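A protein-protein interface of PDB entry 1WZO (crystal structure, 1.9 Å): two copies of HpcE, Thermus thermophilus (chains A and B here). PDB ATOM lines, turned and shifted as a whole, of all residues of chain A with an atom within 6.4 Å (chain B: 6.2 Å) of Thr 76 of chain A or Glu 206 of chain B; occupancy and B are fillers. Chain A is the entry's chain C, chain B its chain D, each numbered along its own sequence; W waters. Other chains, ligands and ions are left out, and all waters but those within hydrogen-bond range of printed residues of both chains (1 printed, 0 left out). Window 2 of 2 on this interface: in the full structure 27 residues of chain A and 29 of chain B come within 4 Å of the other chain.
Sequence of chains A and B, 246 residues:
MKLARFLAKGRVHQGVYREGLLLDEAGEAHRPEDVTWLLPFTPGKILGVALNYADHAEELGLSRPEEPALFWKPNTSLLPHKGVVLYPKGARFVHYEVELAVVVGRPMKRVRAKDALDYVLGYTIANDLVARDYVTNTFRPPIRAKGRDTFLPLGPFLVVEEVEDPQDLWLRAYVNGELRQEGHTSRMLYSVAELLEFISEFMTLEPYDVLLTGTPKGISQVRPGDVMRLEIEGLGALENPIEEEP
Pro 74 of chain A touches Met 203 of chain B.
Thr 76 of chain A touches Lys 45 of chain B.
OG1 of Thr 76 of chain A touches CG of Met 203 of chain B, at 3.7 Å.
Thr 204 of chain B touches Thr 76 of chain A (O to CG2, 3.4 Å).
Thr 76 of chain A touches Glu 206 of chain B.
Met 203 of chain B touches Gly 147 of chain A (CE to O, 3.7 Å).
OD1 of Asp 149 of chain A touches CA of Met 203 of chain B (3.5 Å).
Of the printed residues of chain B, Pro 74 of chain A touches Met 203.
Of the printed residues of chain B, Thr 76 of chain A touches Lys 45, Met 203, Thr 204 and Glu 206.
Of the printed residues of chain B, Asp 149 of chain A touches Met 203 and Thr 204.
Of the printed residues of chain A, Lys 45 of chain B touches Thr 76 (3.3 Å).
Arg 106 of chain B touches none of the printed residues of chain A.
Of the printed residues of chain A, Met 203 of chain B touches Pro 74 (3.9 Å), Thr 76 (3.7 Å), Gly 147 (3.7 Å) and Asp 149 (3.5 Å).
Of the printed residues of chain A, Thr 204 of chain B touches Thr 76 (3.4 Å) and Asp 149 (2.5 Å).
Of the printed residues of chain A, Glu 206 of chain B touches Thr 76.
The nearest printed residue of chain B that does not touch Asp 149 of chain A is Leu 205 of chain B (6.3 Å).
Water W1 lies within hydrogen-bond range of the side-chain amino group (NZ) of Lys 45 of chain B and the backbone NH (N) of Thr 76 of chain A.
The backbone carbonyl oxygen (O) of Pro 74 of chain A lies within hydrogen-bond range of the side-chain hydroxyl (OG) of Ser 77 of chain A (2.5 Å).
The side-chain amino group of Lys 45 of chain B lies within hydrogen-bond range of the backbone carbonyl oxygen of Thr 204 of chain B.
The side-chain amino group (NZ) of Lys 45 of chain B is in salt-bridge range of the side-chain carboxylate (OE1) of Glu 206 of chain B, 3.8 Å away.
The side-chain carboxylate (OD2) of Asp 209 of chain B lies within salt-bridge range of the side-chain amino group (NZ) of Lys 45 of chain B (2.7 Å).
O of Lys 45 of chain B sits at hydrogen-bond distance from N of Val 210 of chain B, at 2.8 Å.
N of Glu 206 of chain B lies within hydrogen-bond range of OD2 of Asp 209 of chain B, at 2.7 Å.
The side-chain carboxylate (OD2) of Asp 149 of chain A lies within hydrogen-bond range of the side-chain hydroxyl (OG1) of Thr 204 of chain B.
No position is printed for both chains.
Of the 8 pairs that touch across the chains among the printed residues, none has its exchanged pair printed and touching as well.
Printed residues of chain A that touch a printed residue of chain B: Pro 74, Thr 76, Gly 147 and Asp 149.
Hydrophobic or aromatic side chains of chain A that line the printed part of chain B: Pro 74.
Of the 14 printed residues of chain B, 4 touch a printed residue of chain A.
Hydrophobic or aromatic side chains of chain B that line the printed part of chain A: Met 203.
Among the printed residues, no Asp or Glu carboxylate lies within 4 Å of a Lys or Arg side-chain nitrogen of the other chain.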
ATOM      1  N   LYS A  73      12.491 -13.918  15.715  1.00  0.00           N
ATOM      2  CA  LYS A  73      13.900 -13.577  15.817  1.00  0.00           C
ATOM      3  C   LYS A  73      14.366 -14.263  17.098  1.00  0.00           C
ATOM      4  O   LYS A  73      13.871 -13.957  18.180  1.00  0.00           O
ATOM      5  CB  LYS A  73      14.087 -12.058  15.939  1.00  0.00           C
ATOM      6  CG  LYS A  73      13.612 -11.258  14.722  1.00  0.00           C
ATOM      7  CD  LYS A  73      14.596 -11.343  13.560  1.00  0.00           C
ATOM      8  CE  LYS A  73      15.889 -10.603  13.872  1.00  0.00           C
ATOM      9  NZ  LYS A  73      16.788 -10.483  12.683  1.00  0.00           N
ATOM     10  N   PRO A  74      15.289 -15.227  16.988  1.00  0.00           N
ATOM     11  CA  PRO A  74      15.764 -15.906  18.196  1.00  0.00           C
ATOM     12  C   PRO A  74      16.576 -14.961  19.082  1.00  0.00           C
ATOM     13  O   PRO A  74      17.180 -13.998  18.597  1.00  0.00           O
ATOM     14  CB  PRO A  74      16.600 -17.056  17.640  1.00  0.00           C
ATOM     15  CG  PRO A  74      17.122 -16.504  16.349  1.00  0.00           C
ATOM     16  CD  PRO A  74      15.901 -15.813  15.782  1.00  0.00           C
ATOM     17  N   ASN A  75      16.582 -15.233  20.382  1.00  0.00           N
ATOM     18  CA  ASN A  75      17.322 -14.397  21.312  1.00  0.00           C
ATOM     19  C   ASN A  75      18.822 -14.453  21.033  1.00  0.00           C
ATOM     20  O   ASN A  75      19.558 -13.537  21.400  1.00  0.00           O
ATOM     21  CB  ASN A  75      17.014 -14.813  22.754  1.00  0.00           C
ATOM     22  CG  ASN A  75      15.573 -14.511  23.150  1.00  0.00           C
ATOM     23  OD1 ASN A  75      15.117 -13.368  23.059  1.00  0.00           O
ATOM     24  ND2 ASN A  75      14.849 -15.535  23.584  1.00  0.00           N
ATOM     25  N   THR A  76      19.276 -15.517  20.371  1.00  0.00           N
ATOM     26  CA  THR A  76      20.692 -15.643  20.039  1.00  0.00           C
ATOM     27  C   THR A  76      21.093 -14.678  18.922  1.00  0.00           C
ATOM     28  O   THR A  76      22.265 -14.568  18.578  1.00  0.00           O
ATOM     29  CB  THR A  76      21.078 -17.097  19.635  1.00  0.00           C
ATOM     30  OG1 THR A  76      20.043 -17.676  18.832  1.00  0.00           O
ATOM     31  CG2 THR A  76      21.301 -17.952  20.879  1.00  0.00           C
ATOM     32  N   SER A  77      20.124 -13.972  18.353  1.00  0.00           N
ATOM     33  CA  SER A  77      20.448 -13.003  17.310  1.00  0.00           C
ATOM     34  C   SER A  77      20.680 -11.635  17.973  1.00  0.00           C
ATOM     35  O   SER A  77      21.311 -10.749  17.394  1.00  0.00           O
ATOM     36  CB  SER A  77      19.314 -12.913  16.277  1.00  0.00           C
ATOM     37  OG  SER A  77      18.118 -12.403  16.847  1.00  0.00           O
ATOM     38  N   LEU A  78      20.188 -11.487  19.203  1.00  0.00           N
ATOM     39  CA  LEU A  78      20.328 -10.240  19.959  1.00  0.00           C
ATOM     40  C   LEU A  78      21.771  -9.776  20.103  1.00  0.00           C
ATOM     41  O   LEU A  78      22.668 -10.564  20.411  1.00  0.00           O
ATOM     42  CB  LEU A  78      19.706 -10.391  21.351  1.00  0.00           C
ATOM     43  CG  LEU A  78      18.175 -10.378  21.397  1.00  0.00           C
ATOM     44  CD1 LEU A  78      17.677 -10.931  22.734  1.00  0.00           C
ATOM     45  CD2 LEU A  78      17.684  -8.963  21.167  1.00  0.00           C
ATOM     46  N   LEU A  79      21.981  -8.481  19.876  1.00  0.00           N
ATOM     47  CA  LEU A  79      23.306  -7.882  19.978  1.00  0.00           C
ATOM     48  C   LEU A  79      23.170  -6.487  20.577  1.00  0.00           C
ATOM     49  O   LEU A  79      22.254  -5.742  20.234  1.00  0.00           O
ATOM     50  CB  LEU A  79      23.950  -7.782  18.595  1.00  0.00           C
ATOM     51  CG  LEU A  79      25.417  -7.351  18.574  1.00  0.00           C
ATOM     52  CD1 LEU A  79      26.281  -8.492  19.064  1.00  0.00           C
ATOM     53  CD2 LEU A  79      25.816  -6.951  17.156  1.00  0.00           C
ATOM     54  N   GLY A 147      17.436 -15.148  11.379  1.00  0.00           N
ATOM     55  CA  GLY A 147      17.649 -15.535  12.763  1.00  0.00           C
ATOM     56  C   GLY A 147      19.066 -15.980  13.058  1.00  0.00           C
ATOM     57  O   GLY A 147      19.301 -16.812  13.936  1.00  0.00           O
ATOM     58  N   ARG A 148      20.020 -15.425  12.322  1.00  0.00           N
ATOM     59  CA  ARG A 148      21.421 -15.772  12.504  1.00  0.00           C
ATOM     60  C   ARG A 148      21.958 -15.073  13.753  1.00  0.00           C
ATOM     61  O   ARG A 148      21.389 -14.079  14.210  1.00  0.00           O
ATOM     62  CB  ARG A 148      22.233 -15.325  11.282  1.00  0.00           C
ATOM     63  CG  ARG A 148      21.590 -15.672   9.946  1.00  0.00           C
ATOM     64  CD  ARG A 148      22.479 -15.256   8.787  1.00  0.00           C
ATOM     65  NE  ARG A 148      23.689 -16.070   8.706  1.00  0.00           N
ATOM     66  CZ  ARG A 148      23.721 -17.324   8.265  1.00  0.00           C
ATOM     67  NH1 ARG A 148      22.608 -17.919   7.861  1.00  0.00           N
ATOM     68  NH2 ARG A 148      24.873 -17.983   8.222  1.00  0.00           N
ATOM     69  N   ASP A 149      23.041 -15.603  14.308  1.00  0.00           N
ATOM     70  CA  ASP A 149      23.656 -14.993  15.481  1.00  0.00           C
ATOM     71  C   ASP A 149      24.070 -13.569  15.118  1.00  0.00           C
ATOM     72  O   ASP A 149      24.525 -13.312  14.002  1.00  0.00           O
ATOM     73  CB  ASP A 149      24.897 -15.781  15.917  1.00  0.00           C
ATOM     74  CG  ASP A 149      24.554 -17.103  16.582  1.00  0.00           C
ATOM     75  OD1 ASP A 149      23.352 -17.419  16.695  1.00  0.00           O
ATOM     76  OD2 ASP A 149      25.491 -17.824  16.990  1.00  0.00           O
ATOM     77  N   THR A 150      23.902 -12.661  16.075  1.00  0.00           N
ATOM     78  CA  THR A 150      24.242 -11.243  15.946  1.00  0.00           C
ATOM     79  C   THR A 150      23.386 -10.458  14.957  1.00  0.00           C
ATOM     80  O   THR A 150      23.654  -9.281  14.712  1.00  0.00           O
ATOM     81  CB  THR A 150      25.731 -11.037  15.559  1.00  0.00           C
ATOM     82  OG1 THR A 150      25.922 -11.329  14.170  1.00  0.00           O
ATOM     83  CG2 THR A 150      26.630 -11.942  16.387  1.00  0.00           C
ATOM     84  N   PHE A 151      22.349 -11.080  14.403  1.00  0.00           N
ATOM     85  CA  PHE A 151      21.517 -10.365  13.443  1.00  0.00           C
ATOM     86  C   PHE A 151      20.403  -9.502  14.011  1.00  0.00           C
ATOM     87  O   PHE A 151      19.463  -9.160  13.298  1.00  0.00           O
ATOM     88  CB  PHE A 151      20.934 -11.319  12.392  1.00  0.00           C
ATOM     89  CG  PHE A 151      21.739 -11.377  11.117  1.00  0.00           C
ATOM     90  CD1 PHE A 151      21.128 -11.691   9.903  1.00  0.00           C
ATOM     91  CD2 PHE A 151      23.110 -11.117  11.130  1.00  0.00           C
ATOM     92  CE1 PHE A 151      21.868 -11.745   8.722  1.00  0.00           C
ATOM     93  CE2 PHE A 151      23.862 -11.169   9.954  1.00  0.00           C
ATOM     94  CZ  PHE A 151      23.239 -11.483   8.747  1.00  0.00           C
ATOM     95  N   LYS B  45      14.586 -21.841  23.422  1.00  0.00           N
ATOM     96  CA  LYS B  45      13.850 -21.614  22.181  1.00  0.00           C
ATOM     97  C   LYS B  45      13.435 -22.966  21.602  1.00  0.00           C
ATOM     98  O   LYS B  45      14.111 -23.969  21.803  1.00  0.00           O
ATOM     99  CB  LYS B  45      14.676 -20.807  21.167  1.00  0.00           C
ATOM    100  CG  LYS B  45      16.135 -21.212  21.002  1.00  0.00           C
ATOM    101  CD  LYS B  45      16.838 -20.261  20.024  1.00  0.00           C
ATOM    102  CE  LYS B  45      18.303 -20.629  19.813  1.00  0.00           C
ATOM    103  NZ  LYS B  45      19.109 -20.448  21.062  1.00  0.00           N
ATOM    104  N   VAL B 104      18.425 -30.064  23.715  1.00  0.00           N
ATOM    105  CA  VAL B 104      19.855 -29.786  23.648  1.00  0.00           C
ATOM    106  C   VAL B 104      20.477 -29.790  25.043  1.00  0.00           C
ATOM    107  O   VAL B 104      19.885 -29.279  25.995  1.00  0.00           O
ATOM    108  CB  VAL B 104      20.111 -28.421  22.976  1.00  0.00           C
ATOM    109  CG1 VAL B 104      21.604 -28.119  22.947  1.00  0.00           C
ATOM    110  CG2 VAL B 104      19.534 -28.431  21.564  1.00  0.00           C
ATOM    111  N   GLY B 105      21.668 -30.374  25.153  1.00  0.00           N
ATOM    112  CA  GLY B 105      22.354 -30.452  26.433  1.00  0.00           C
ATOM    113  C   GLY B 105      23.606 -29.595  26.546  1.00  0.00           C
ATOM    114  O   GLY B 105      24.002 -29.219  27.651  1.00  0.00           O
ATOM    115  N   ARG B 106      24.240 -29.299  25.413  1.00  0.00           N
ATOM    116  CA  ARG B 106      25.450 -28.472  25.395  1.00  0.00           C
ATOM    117  C   ARG B 106      25.359 -27.446  24.269  1.00  0.00           C
ATOM    118  O   ARG B 106      24.716 -27.696  23.253  1.00  0.00           O
ATOM    119  CB  ARG B 106      26.697 -29.336  25.194  1.00  0.00           C
ATOM    120  CG  ARG B 106      27.029 -30.257  26.357  1.00  0.00           C
ATOM    121  CD  ARG B 106      28.387 -30.913  26.152  1.00  0.00           C
ATOM    122  NE  ARG B 106      28.404 -31.794  24.988  1.00  0.00           N
ATOM    123  CZ  ARG B 106      29.425 -31.891  24.139  1.00  0.00           C
ATOM    124  NH1 ARG B 106      30.515 -31.156  24.317  1.00  0.00           N
ATOM    125  NH2 ARG B 106      29.358 -32.727  23.112  1.00  0.00           N
ATOM    126  N   PRO B 107      26.002 -26.275  24.435  1.00  0.00           N
ATOM    127  CA  PRO B 107      25.956 -25.240  23.394  1.00  0.00           C
ATOM    128  C   PRO B 107      26.395 -25.781  22.034  1.00  0.00           C
ATOM    129  O   PRO B 107      27.424 -26.453  21.930  1.00  0.00           O
ATOM    130  CB  PRO B 107      26.908 -24.170  23.926  1.00  0.00           C
ATOM    131  CG  PRO B 107      26.804 -24.333  25.425  1.00  0.00           C
ATOM    132  CD  PRO B 107      26.839 -25.839  25.568  1.00  0.00           C
ATOM    133  N   MET B 108      25.616 -25.484  20.999  1.00  0.00           N
ATOM    134  CA  MET B 108      25.934 -25.959  19.658  1.00  0.00           C
ATOM    135  C   MET B 108      26.059 -24.833  18.640  1.00  0.00           C
ATOM    136  O   MET B 108      25.155 -24.010  18.492  1.00  0.00           O
ATOM    137  CB  MET B 108      24.862 -26.936  19.155  1.00  0.00           C
ATOM    138  CG  MET B 108      24.591 -28.137  20.045  1.00  0.00           C
ATOM    139  SD  MET B 108      23.430 -29.310  19.268  1.00  0.00           S
ATOM    140  CE  MET B 108      21.958 -28.464  19.412  1.00  0.00           C
ATOM    141  N   MET B 203      22.819 -20.712  13.848  1.00  0.00           N
ATOM    142  CA  MET B 203      22.153 -20.321  15.087  1.00  0.00           C
ATOM    143  C   MET B 203      22.693 -21.118  16.266  1.00  0.00           C
ATOM    144  O   MET B 203      22.702 -22.349  16.237  1.00  0.00           O
ATOM    145  CB  MET B 203      20.645 -20.562  14.969  1.00  0.00           C
ATOM    146  CG  MET B 203      19.854 -20.217  16.215  1.00  0.00           C
ATOM    147  SD  MET B 203      18.137 -20.791  16.148  1.00  0.00           S
ATOM    148  CE  MET B 203      17.556 -19.973  14.633  1.00  0.00           C
ATOM    149  N   THR B 204      23.146 -20.421  17.302  1.00  0.00           N
ATOM    150  CA  THR B 204      23.670 -21.106  18.471  1.00  0.00           C
ATOM    151  C   THR B 204      22.517 -21.726  19.249  1.00  0.00           C
ATOM    152  O   THR B 204      21.533 -21.056  19.564  1.00  0.00           O
ATOM    153  CB  THR B 204      24.435 -20.147  19.417  1.00  0.00           C
ATOM    154  OG1 THR B 204      25.602 -19.642  18.758  1.00  0.00           O
ATOM    155  CG2 THR B 204      24.865 -20.888  20.682  1.00  0.00           C
ATOM    156  N   LEU B 205      22.633 -23.014  19.539  1.00  0.00           N
ATOM    157  CA  LEU B 205      21.604 -23.701  20.300  1.00  0.00           C
ATOM    158  C   LEU B 205      22.149 -23.856  21.710  1.00  0.00           C
ATOM    159  O   LEU B 205      23.272 -24.329  21.907  1.00  0.00           O
ATOM    160  CB  LEU B 205      21.294 -25.065  19.679  1.00  0.00           C
ATOM    161  CG  LEU B 205      20.702 -24.985  18.263  1.00  0.00           C
ATOM    162  CD1 LEU B 205      20.352 -26.380  17.772  1.00  0.00           C
ATOM    163  CD2 LEU B 205      19.460 -24.101  18.265  1.00  0.00           C
ATOM    164  N   GLU B 206      21.358 -23.434  22.687  1.00  0.00           N
ATOM    165  CA  GLU B 206      21.774 -23.493  24.083  1.00  0.00           C
ATOM    166  C   GLU B 206      21.115 -24.637  24.843  1.00  0.00           C
ATOM    167  O   GLU B 206      20.076 -25.147  24.430  1.00  0.00           O
ATOM    168  CB  GLU B 206      21.444 -22.162  24.754  1.00  0.00           C
ATOM    169  CG  GLU B 206      22.003 -20.960  23.996  1.00  0.00           C
ATOM    170  CD  GLU B 206      21.436 -19.645  24.485  1.00  0.00           C
ATOM    171  OE1 GLU B 206      20.195 -19.514  24.533  1.00  0.00           O
ATOM    172  OE2 GLU B 206      22.227 -18.739  24.813  1.00  0.00           O
ATOM    173  N   PRO B 207      21.722 -25.067  25.963  1.00  0.00           N
ATOM    174  CA  PRO B 207      21.123 -26.162  26.729  1.00  0.00           C
ATOM    175  C   PRO B 207      19.648 -25.868  27.011  1.00  0.00           C
ATOM    176  O   PRO B 207      19.281 -24.742  27.349  1.00  0.00           O
ATOM    177  CB  PRO B 207      21.979 -26.199  27.994  1.00  0.00           C
ATOM    178  CG  PRO B 207      23.341 -25.818  27.463  1.00  0.00           C
ATOM    179  CD  PRO B 207      23.001 -24.642  26.560  1.00  0.00           C
ATOM    180  N   TYR B 208      18.817 -26.894  26.841  1.00  0.00           N
ATOM    181  CA  TYR B 208      17.366 -26.829  27.033  1.00  0.00           C
ATOM    182  C   TYR B 208      16.589 -26.205  25.874  1.00  0.00           C
ATOM    183  O   TYR B 208      15.386 -25.948  25.994  1.00  0.00           O
ATOM    184  CB  TYR B 208      17.010 -26.146  28.359  1.00  0.00           C
ATOM    185  CG  TYR B 208      17.505 -26.940  29.553  1.00  0.00           C
ATOM    186  CD1 TYR B 208      18.464 -26.415  30.416  1.00  0.00           C
ATOM    187  CD2 TYR B 208      17.061 -28.243  29.777  1.00  0.00           C
ATOM    188  CE1 TYR B 208      18.976 -27.175  31.477  1.00  0.00           C
ATOM    189  CE2 TYR B 208      17.566 -29.013  30.829  1.00  0.00           C
ATOM    190  CZ  TYR B 208      18.522 -28.468  31.671  1.00  0.00           C
ATOM    191  OH  TYR B 208      19.029 -29.226  32.699  1.00  0.00           O
ATOM    192  N   ASP B 209      17.267 -25.940  24.758  1.00  0.00           N
ATOM    193  CA  ASP B 209      16.550 -25.437  23.588  1.00  0.00           C
ATOM    194  C   ASP B 209      15.925 -26.727  23.074  1.00  0.00           C
ATOM    195  O   ASP B 209      16.462 -27.808  23.333  1.00  0.00           O
ATOM    196  CB  ASP B 209      17.500 -24.856  22.528  1.00  0.00           C
ATOM    197  CG  ASP B 209      17.819 -23.393  22.773  1.00  0.00           C
ATOM    198  OD1 ASP B 209      17.141 -22.776  23.627  1.00  0.00           O
ATOM    199  OD2 ASP B 209      18.736 -22.860  22.105  1.00  0.00           O
ATOM    200  N   VAL B 210      14.810 -26.634  22.357  1.00  0.00           N
ATOM    201  CA  VAL B 210      14.148 -27.843  21.876  1.00  0.00           C
ATOM    202  C   VAL B 210      13.934 -27.878  20.372  1.00  0.00           C
ATOM    203  O   VAL B 210      13.663 -26.852  19.742  1.00  0.00           O
ATOM    204  CB  VAL B 210      12.787 -28.025  22.591  1.00  0.00           C
ATOM    205  CG1 VAL B 210      12.084 -29.297  22.107  1.00  0.00           C
ATOM    206  CG2 VAL B 210      13.015 -28.110  24.104  1.00  0.00           C
HETATM  207  O   HOH W   1      18.132 -17.964  22.117  1.00  0.00           O
